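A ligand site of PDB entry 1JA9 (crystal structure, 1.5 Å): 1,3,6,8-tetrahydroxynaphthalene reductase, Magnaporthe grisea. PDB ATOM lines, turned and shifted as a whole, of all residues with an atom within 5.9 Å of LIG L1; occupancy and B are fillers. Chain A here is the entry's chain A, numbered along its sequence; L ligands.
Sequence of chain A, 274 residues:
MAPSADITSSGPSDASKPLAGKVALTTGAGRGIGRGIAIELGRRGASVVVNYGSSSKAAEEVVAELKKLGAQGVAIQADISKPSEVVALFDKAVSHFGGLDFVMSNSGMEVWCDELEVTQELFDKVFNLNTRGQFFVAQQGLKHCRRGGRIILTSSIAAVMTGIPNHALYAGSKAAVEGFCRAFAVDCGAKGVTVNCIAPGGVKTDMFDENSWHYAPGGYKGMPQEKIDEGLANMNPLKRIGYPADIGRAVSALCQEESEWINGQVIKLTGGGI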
ATOM      1  N   GLU A 110      -1.214  22.978   8.113  1.00  0.00           N
ATOM      2  CA  GLU A 110       0.210  22.720   8.306  1.00  0.00           C
ATOM      3  C   GLU A 110       0.280  21.204   8.472  1.00  0.00           C
ATOM      4  O   GLU A 110      -0.736  20.525   8.672  1.00  0.00           O
ATOM      5  CB  GLU A 110       0.715  23.379   9.590  1.00  0.00           C
ATOM      6  CG  GLU A 110       1.648  24.563   9.324  1.00  0.00           C
ATOM      7  CD  GLU A 110       3.049  24.145   8.835  1.00  0.00           C
ATOM      8  OE1 GLU A 110       3.996  24.943   9.037  1.00  0.00           O
ATOM      9  OE2 GLU A 110       3.203  23.037   8.295  1.00  0.00           O
ATOM     10  N   SER A 155       0.396  30.538  -0.959  1.00  0.00           N
ATOM     11  CA  SER A 155       1.528  29.639  -0.833  1.00  0.00           C
ATOM     12  C   SER A 155       2.076  29.877   0.625  1.00  0.00           C
ATOM     13  O   SER A 155       1.287  29.972   1.577  1.00  0.00           O
ATOM     14  CB  SER A 155       2.574  30.009  -1.889  1.00  0.00           C
ATOM     15  OG  SER A 155       3.633  29.080  -1.871  1.00  0.00           O
ATOM     16  N   SER A 156       3.393  29.983   0.771  1.00  0.00           N
ATOM     17  CA  SER A 156       4.047  30.231   2.060  1.00  0.00           C
ATOM     18  C   SER A 156       5.521  30.352   1.777  1.00  0.00           C
ATOM     19  O   SER A 156       6.006  29.738   0.820  1.00  0.00           O
ATOM     20  CB  SER A 156       3.867  29.035   3.038  1.00  0.00           C
ATOM     21  OG  SER A 156       4.735  29.162   4.176  1.00  0.00           O
ATOM     22  N   ILE A 157       6.266  31.084   2.610  1.00  0.00           N
ATOM     23  CA  ILE A 157       7.721  31.132   2.371  1.00  0.00           C
ATOM     24  C   ILE A 157       8.311  29.728   2.620  1.00  0.00           C
ATOM     25  O   ILE A 157       9.388  29.416   2.141  1.00  0.00           O
ATOM     26  CB  ILE A 157       8.462  32.154   3.237  1.00  0.00           C
ATOM     27  CG1 ILE A 157       8.199  31.893   4.721  1.00  0.00           C
ATOM     28  CG2 ILE A 157       8.060  33.542   2.805  1.00  0.00           C
ATOM     29  CD1 ILE A 157       8.939  32.889   5.601  1.00  0.00           C
ATOM     30  N   ALA A 158       7.571  28.878   3.335  1.00  0.00           N
ATOM     31  CA  ALA A 158       8.056  27.530   3.561  1.00  0.00           C
ATOM     32  C   ALA A 158       8.182  26.755   2.226  1.00  0.00           C
ATOM     33  O   ALA A 158       8.912  25.752   2.154  1.00  0.00           O
ATOM     34  CB  ALA A 158       7.144  26.766   4.546  1.00  0.00           C
ATOM     35  N   MET A 161      11.796  27.669   1.483  1.00  0.00           N
ATOM     36  CA  MET A 161      12.801  27.696   2.560  1.00  0.00           C
ATOM     37  C   MET A 161      13.662  26.449   2.553  1.00  0.00           C
ATOM     38  O   MET A 161      13.280  25.403   2.046  1.00  0.00           O
ATOM     39  CB  MET A 161      12.157  27.760   3.935  1.00  0.00           C
ATOM     40  CG  MET A 161      11.740  29.132   4.349  1.00  0.00           C
ATOM     41  SD  MET A 161      10.893  28.969   5.960  1.00  0.00           S
ATOM     42  CE  MET A 161      12.408  28.871   6.992  1.00  0.00           C
ATOM     43  N   HIS A 167       8.970  18.204   6.516  1.00  0.00           N
ATOM     44  CA  HIS A 167       7.993  19.138   5.985  1.00  0.00           C
ATOM     45  C   HIS A 167       7.753  19.043   4.486  1.00  0.00           C
ATOM     46  O   HIS A 167       7.274  20.000   3.885  1.00  0.00           O
ATOM     47  CB  HIS A 167       8.502  20.539   6.325  1.00  0.00           C
ATOM     48  CG  HIS A 167       7.413  21.534   6.537  1.00  0.00           C
ATOM     49  ND1 HIS A 167       7.545  22.865   6.189  1.00  0.00           N
ATOM     50  CD2 HIS A 167       6.226  21.430   7.176  1.00  0.00           C
ATOM     51  CE1 HIS A 167       6.491  23.539   6.613  1.00  0.00           C
ATOM     52  NE2 HIS A 167       5.676  22.688   7.214  1.00  0.00           N
ATOM     53  N   TYR A 170       4.013  19.768   3.251  1.00  0.00           N
ATOM     54  CA  TYR A 170       3.621  21.178   3.269  1.00  0.00           C
ATOM     55  C   TYR A 170       4.369  21.976   2.201  1.00  0.00           C
ATOM     56  O   TYR A 170       3.750  22.689   1.414  1.00  0.00           O
ATOM     57  CB  TYR A 170       3.857  21.791   4.642  1.00  0.00           C
ATOM     58  CG  TYR A 170       3.266  23.174   4.777  1.00  0.00           C
ATOM     59  CD1 TYR A 170       1.899  23.342   5.053  1.00  0.00           C
ATOM     60  CD2 TYR A 170       4.081  24.333   4.682  1.00  0.00           C
ATOM     61  CE1 TYR A 170       1.357  24.629   5.236  1.00  0.00           C
ATOM     62  CE2 TYR A 170       3.546  25.614   4.871  1.00  0.00           C
ATOM     63  CZ  TYR A 170       2.181  25.752   5.151  1.00  0.00           C
ATOM     64  OH  TYR A 170       1.635  27.006   5.363  1.00  0.00           O
ATOM     65  N   LYS A 174       2.408  23.635  -1.133  1.00  0.00           N
ATOM     66  CA  LYS A 174       2.403  25.082  -1.333  1.00  0.00           C
ATOM     67  C   LYS A 174       3.148  25.467  -2.623  1.00  0.00           C
ATOM     68  O   LYS A 174       2.694  26.317  -3.396  1.00  0.00           O
ATOM     69  CB  LYS A 174       3.003  25.764  -0.120  1.00  0.00           C
ATOM     70  CG  LYS A 174       2.162  25.612   1.163  1.00  0.00           C
ATOM     71  CD  LYS A 174       0.776  26.195   0.952  1.00  0.00           C
ATOM     72  CE  LYS A 174       0.169  26.626   2.297  1.00  0.00           C
ATOM     73  NZ  LYS A 174      -1.144  27.303   2.149  1.00  0.00           N
ATOM     74  N   PRO A 200       3.113  34.261   2.679  1.00  0.00           N
ATOM     75  CA  PRO A 200       3.387  34.906   3.964  1.00  0.00           C
ATOM     76  C   PRO A 200       4.504  34.261   4.778  1.00  0.00           C
ATOM     77  O   PRO A 200       4.846  33.083   4.589  1.00  0.00           O
ATOM     78  CB  PRO A 200       2.044  34.765   4.731  1.00  0.00           C
ATOM     79  CG  PRO A 200       1.015  34.531   3.624  1.00  0.00           C
ATOM     80  CD  PRO A 200       1.786  33.615   2.691  1.00  0.00           C
ATOM     81  N   GLY A 201       5.072  35.101   5.651  1.00  0.00           N
ATOM     82  CA  GLY A 201       6.039  34.643   6.628  1.00  0.00           C
ATOM     83  C   GLY A 201       5.111  34.362   7.814  1.00  0.00           C
ATOM     84  O   GLY A 201       3.884  34.317   7.622  1.00  0.00           O
ATOM     85  N   GLY A 202       5.636  34.233   9.030  1.00  0.00           N
ATOM     86  CA  GLY A 202       4.801  33.928  10.193  1.00  0.00           C
ATOM     87  C   GLY A 202       3.741  34.988  10.453  1.00  0.00           C
ATOM     88  O   GLY A 202       4.059  36.180  10.446  1.00  0.00           O
ATOM     89  N   VAL A 203       2.497  34.579  10.693  1.00  0.00           N
ATOM     90  CA  VAL A 203       1.400  35.521  10.955  1.00  0.00           C
ATOM     91  C   VAL A 203       0.642  34.954  12.171  1.00  0.00           C
ATOM     92  O   VAL A 203       0.239  33.797  12.149  1.00  0.00           O
ATOM     93  CB  VAL A 203       0.419  35.592   9.761  1.00  0.00           C
ATOM     94  CG1 VAL A 203      -0.716  36.618  10.058  1.00  0.00           C
ATOM     95  CG2 VAL A 203       1.176  36.008   8.470  1.00  0.00           C
ATOM     96  N   MET A 207      -2.772  28.562  13.590  1.00  0.00           N
ATOM     97  CA  MET A 207      -1.733  27.755  12.943  1.00  0.00           C
ATOM     98  C   MET A 207      -0.345  28.197  13.427  1.00  0.00           C
ATOM     99  O   MET A 207       0.534  27.352  13.666  1.00  0.00           O
ATOM    100  CB  MET A 207      -1.802  27.883  11.426  1.00  0.00           C
ATOM    101  CG  MET A 207      -0.722  27.092  10.690  1.00  0.00           C
ATOM    102  SD  MET A 207      -0.780  27.361   8.895  1.00  0.00           S
ATOM    103  CE  MET A 207      -2.330  26.482   8.465  1.00  0.00           C
ATOM    104  N   PHE A 208      -0.148  29.490  13.571  1.00  0.00           N
ATOM    105  CA  PHE A 208       1.140  30.037  14.019  1.00  0.00           C
ATOM    106  C   PHE A 208       1.416  29.597  15.463  1.00  0.00           C
ATOM    107  O   PHE A 208       2.516  29.172  15.800  1.00  0.00           O
ATOM    108  CB  PHE A 208       1.097  31.554  13.935  1.00  0.00           C
ATOM    109  CG  PHE A 208       2.313  32.257  14.475  1.00  0.00           C
ATOM    110  CD1 PHE A 208       3.308  32.734  13.605  1.00  0.00           C
ATOM    111  CD2 PHE A 208       2.427  32.526  15.854  1.00  0.00           C
ATOM    112  CE1 PHE A 208       4.397  33.465  14.068  1.00  0.00           C
ATOM    113  CE2 PHE A 208       3.505  33.257  16.348  1.00  0.00           C
ATOM    114  CZ  PHE A 208       4.507  33.738  15.455  1.00  0.00           C
ATOM    115  N   ASN A 211       2.405  25.912  15.304  1.00  0.00           N
ATOM    116  CA  ASN A 211       3.563  25.539  14.504  1.00  0.00           C
ATOM    117  C   ASN A 211       4.785  26.440  14.480  1.00  0.00           C
ATOM    118  O   ASN A 211       5.804  26.041  13.893  1.00  0.00           O
ATOM    119  CB  ASN A 211       3.093  25.366  13.053  1.00  0.00           C
ATOM    120  CG  ASN A 211       2.037  24.276  12.895  1.00  0.00           C
ATOM    121  OD1 ASN A 211       2.367  23.087  12.745  1.00  0.00           O
ATOM    122  ND2 ASN A 211       0.752  24.662  12.940  1.00  0.00           N
ATOM    123  N   SER A 212       4.714  27.641  15.051  1.00  0.00           N
ATOM    124  CA  SER A 212       5.818  28.592  14.978  1.00  0.00           C
ATOM    125  C   SER A 212       7.162  28.152  15.563  1.00  0.00           C
ATOM    126  O   SER A 212       8.210  28.620  15.117  1.00  0.00           O
ATOM    127  CB  SER A 212       5.403  29.947  15.558  1.00  0.00           C
ATOM    128  OG  SER A 212       4.886  29.825  16.892  1.00  0.00           O
ATOM    129  N   TYR A 215       9.893  27.203  13.200  1.00  0.00           N
ATOM    130  CA  TYR A 215      10.514  28.286  12.433  1.00  0.00           C
ATOM    131  C   TYR A 215      11.383  29.245  13.251  1.00  0.00           C
ATOM    132  O   TYR A 215      12.159  30.015  12.691  1.00  0.00           O
ATOM    133  CB  TYR A 215       9.410  29.076  11.727  1.00  0.00           C
ATOM    134  CG  TYR A 215       8.582  28.212  10.789  1.00  0.00           C
ATOM    135  CD1 TYR A 215       7.402  27.577  11.226  1.00  0.00           C
ATOM    136  CD2 TYR A 215       8.942  28.064   9.445  1.00  0.00           C
ATOM    137  CE1 TYR A 215       6.614  26.841  10.366  1.00  0.00           C
ATOM    138  CE2 TYR A 215       8.151  27.328   8.572  1.00  0.00           C
ATOM    139  CZ  TYR A 215       6.989  26.735   9.030  1.00  0.00           C
ATOM    140  OH  TYR A 215       6.188  26.090   8.128  1.00  0.00           O
ATOM    141  N   LEU A 232      11.132  35.553  16.667  1.00  0.00           N
ATOM    142  CA  LEU A 232      10.704  35.843  15.293  1.00  0.00           C
ATOM    143  C   LEU A 232      10.706  37.357  15.023  1.00  0.00           C
ATOM    144  O   LEU A 232      11.264  37.818  14.028  1.00  0.00           O
ATOM    145  CB  LEU A 232       9.351  35.204  15.014  1.00  0.00           C
ATOM    146  CG  LEU A 232       9.369  33.670  14.930  1.00  0.00           C
ATOM    147  CD1 LEU A 232       7.971  33.127  14.798  1.00  0.00           C
ATOM    148  CD2 LEU A 232      10.215  33.219  13.761  1.00  0.00           C
ATOM    149  N   ILE A 274      10.867  36.484   8.650  1.00  0.00           N
ATOM    150  CA  ILE A 274      10.666  35.044   8.440  1.00  0.00           C
ATOM    151  C   ILE A 274       9.315  34.496   8.907  1.00  0.00           C
ATOM    152  O   ILE A 274       9.224  33.268   9.107  1.00  0.00           O
ATOM    153  CB  ILE A 274      11.768  34.229   9.159  1.00  0.00           C
ATOM    154  CG1 ILE A 274      11.811  34.587  10.655  1.00  0.00           C
ATOM    155  CG2 ILE A 274      13.095  34.504   8.506  1.00  0.00           C
ATOM    156  CD1 ILE A 274      12.934  33.891  11.450  1.00  0.00           C
ATOM    157  OXT ILE A 274       8.387  35.294   9.121  1.00  0.00           O
HETATM  158  C1  LIG L   1       4.810  30.030  11.752  1.00  0.00           C
HETATM  159  C2  LIG L   1       4.411  29.539  10.491  1.00  0.00           C
HETATM  160  C3  LIG L   1       5.214  29.910   9.375  1.00  0.00           C
HETATM  161  C4  LIG L   1       6.352  30.730   9.483  1.00  0.00           C
HETATM  162  C5  LIG L   1       6.941  30.912   8.086  1.00  0.00           C
HETATM  163  C6  LIG L   1       5.943  30.072   7.225  1.00  0.00           C
HETATM  164  N1  LIG L   1       4.969  29.532   8.100  1.00  0.00           N
HETATM  165  C7  LIG L   1       3.907  28.736   7.816  1.00  0.00           C
HETATM  166  O1  LIG L   1       3.676  28.384   6.605  1.00  0.00           O
HETATM  167  C8  LIG L   1       3.049  28.309   8.868  1.00  0.00           C
HETATM  168  C9  LIG L   1       3.280  28.696  10.206  1.00  0.00           C
HETATM  169  C10 LIG L   1       6.745  31.227  10.739  1.00  0.00           C
HETATM  170  C11 LIG L   1       5.965  30.864  11.871  1.00  0.00           C
HETATM  171  P1  LG2 L   2      -5.471  28.489  10.741  1.00  0.00           P
HETATM  172  O1  LG2 L   2      -5.104  27.071  10.947  1.00  0.00           O
HETATM  173  O2  LG2 L   2      -5.472  29.506  11.801  1.00  0.00           O
HETATM  174  O3  LG2 L   2      -6.902  28.562   9.972  1.00  0.00           O
HETATM  175  C1  LG2 L   2      -6.954  27.975   8.646  1.00  0.00           C
HETATM  176  C2  LG2 L   2      -8.258  28.163   7.876  1.00  0.00           C
HETATM  177  O4  LG2 L   2      -8.349  27.110   6.908  1.00  0.00           O
HETATM  178  C3  LG2 L   2      -9.431  28.133   8.793  1.00  0.00           C
HETATM  179  O5  LG2 L   2     -10.352  29.219   8.491  1.00  0.00           O
HETATM  180  C4  LG2 L   2     -10.128  26.875   8.374  1.00  0.00           C
HETATM  181  O6  LG2 L   2     -11.556  27.019   8.663  1.00  0.00           O
HETATM  182  C5  LG2 L   2      -9.699  26.742   6.929  1.00  0.00           C
HETATM  183  N1  LG2 L   2     -10.028  25.399   6.471  1.00  0.00           N
HETATM  184  C6  LG2 L   2      -9.329  24.292   6.866  1.00  0.00           C
HETATM  185  N2  LG2 L   2      -9.827  23.219   6.267  1.00  0.00           N
HETATM  186  C7  LG2 L   2     -10.839  23.687   5.520  1.00  0.00           C
HETATM  187  C8  LG2 L   2     -11.675  22.921   4.706  1.00  0.00           C
HETATM  188  N3  LG2 L   2     -11.535  21.592   4.533  1.00  0.00           N
HETATM  189  N4  LG2 L   2     -12.629  23.614   4.039  1.00  0.00           N
HETATM  190  C9  LG2 L   2     -12.754  24.963   4.159  1.00  0.00           C
HETATM  191  N5  LG2 L   2     -11.945  25.681   4.940  1.00  0.00           N
HETATM  192  C10 LG2 L   2     -10.976  25.063   5.644  1.00  0.00           C
HETATM  193  O7  LG2 L   2      -4.618  29.083   9.476  1.00  0.00           O
HETATM  194  P2  LG2 L   2      -3.933  30.477   9.106  1.00  0.00           P
HETATM  195  O8  LG2 L   2      -5.070  31.449   9.058  1.00  0.00           O
HETATM  196  O9  LG2 L   2      -2.784  30.762   9.955  1.00  0.00           O
HETATM  197  O10 LG2 L   2      -3.439  30.201   7.607  1.00  0.00           O
HETATM  198  C11 LG2 L   2      -4.290  30.464   6.468  1.00  0.00           C
HETATM  199  C12 LG2 L   2      -3.518  30.177   5.181  1.00  0.00           C
HETATM  200  O11 LG2 L   2      -2.230  30.867   5.202  1.00  0.00           O
HETATM  201  C13 LG2 L   2      -3.156  28.718   5.021  1.00  0.00           C
HETATM  202  O12 LG2 L   2      -3.204  28.330   3.649  1.00  0.00           O
HETATM  203  C14 LG2 L   2      -1.738  28.594   5.573  1.00  0.00           C
HETATM  204  O13 LG2 L   2      -1.005  27.463   5.079  1.00  0.00           O
HETATM  205  C15 LG2 L   2      -1.195  29.904   5.048  1.00  0.00           C
HETATM  206  N6  LG2 L   2      -0.036  30.426   5.772  1.00  0.00           N
HETATM  207  C16 LG2 L   2      -0.070  30.754   7.146  1.00  0.00           C
HETATM  208  C17 LG2 L   2       1.060  31.299   7.761  1.00  0.00           C
HETATM  209  C18 LG2 L   2       1.087  31.681   9.226  1.00  0.00           C
HETATM  210  O14 LG2 L   2       2.145  32.039   9.723  1.00  0.00           O
HETATM  211  N7  LG2 L   2      -0.065  31.649   9.912  1.00  0.00           N
HETATM  212  C19 LG2 L   2       2.229  31.516   7.017  1.00  0.00           C
HETATM  213  C20 LG2 L   2       2.277  31.203   5.642  1.00  0.00           C
HETATM  214  C21 LG2 L   2       1.133  30.652   5.000  1.00  0.00           C
HETATM  215  P3  LG2 L   2     -12.392  25.891   9.419  1.00  0.00           P
HETATM  216  O15 LG2 L   2     -12.117  26.107  10.830  1.00  0.00           O
HETATM  217  O16 LG2 L   2     -12.078  24.526   8.949  1.00  0.00           O
HETATM  218  O17 LG2 L   2     -13.841  26.192   9.169  1.00  0.00           O
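The backbone carbonyl oxygen (O) of Met 207 sits at hydrogen-bond distance from the side-chain amide nitrogen (ND2) of Asn 211 (2.8 Å). The side-chain hydroxyl (OG) of Ser 156 lies close to the backbone NH (N) of Ala 158, at 3.0 Å. The side-chain carboxylate (OE2) of Glu 110 is in hydrogen-bond range of a ring nitrogen (NE2) of His 167, at 2.7 Å. OH of Tyr 215 is in hydrogen-bond range of OE1 of Glu 110 (2.6 Å). The backbone carbonyl oxygen (O) of Pro 200 lies within hydrogen-bond range of the backbone NH (N) of Ile 157 (3.2 Å). The side-chain hydroxyl of Ser 212 is in hydrogen-bond range of the backbone carbonyl oxygen of Phe 208 (2.7 Å). The backbone NH of Gly 202 lies within hydrogen-bond range of the chain-end carboxylate of Ile 274 (2.9 Å).
N7 of LG2 L2 lies within hydrogen-bond range of O of Val 203, at 3.1 Å. O12 of LG2 L2 sits at hydrogen-bond distance from NZ of Lys 174 (2.7 Å). OG of Ser 156 sits at hydrogen-bond distance from O1 of LIG L1 (2.8 Å). The backbone NH (N) of Val 203 lies within hydrogen-bond range of an oxygen (O14) of LG2 L2 (2.7 Å). An oxygen (O13) of LG2 L2 lies within hydrogen-bond range of the side-chain hydroxyl (OH) of Tyr 170, 2.7 Å away. An oxygen (O1) of LIG L1 lies within hydrogen-bond range of the side-chain hydroxyl (OH) of Tyr 170, at 2.8 Å. The backbone NH (N) of Met 207 is in hydrogen-bond range of an oxygen (O2) of LG2 L2, 3.4 Å away.
Residues that only touch LIG L1: Gly 202 (3.4 Å), Ile 274 (3.4 Å), Tyr 215 (3.5 Å), Glu 110 (3.5 Å), Phe 208 (3.6 Å), Ser 212 (3.7 Å), Ile 157 (3.7 Å), Gly 201 (3.9 Å) and Met 207 (3.9 Å). Hydrophobic or aromatic side chains that line LIG L1: Ile 157, Tyr 170, Met 207, Phe 208 and Tyr 215. Within 4 Å of LIG L1: Glu 110, Ser 156, Ile 157, Tyr 170, Gly 201, Gly 202, Met 207, Phe 208, Ser 212, Tyr 215 and Ile 274. Along chain A the residues within 4 Å of LIG L1 span positions 110 to 274. The nearest printed residue that does not touch LIG L1 is Pro 200 (4.1 Å).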
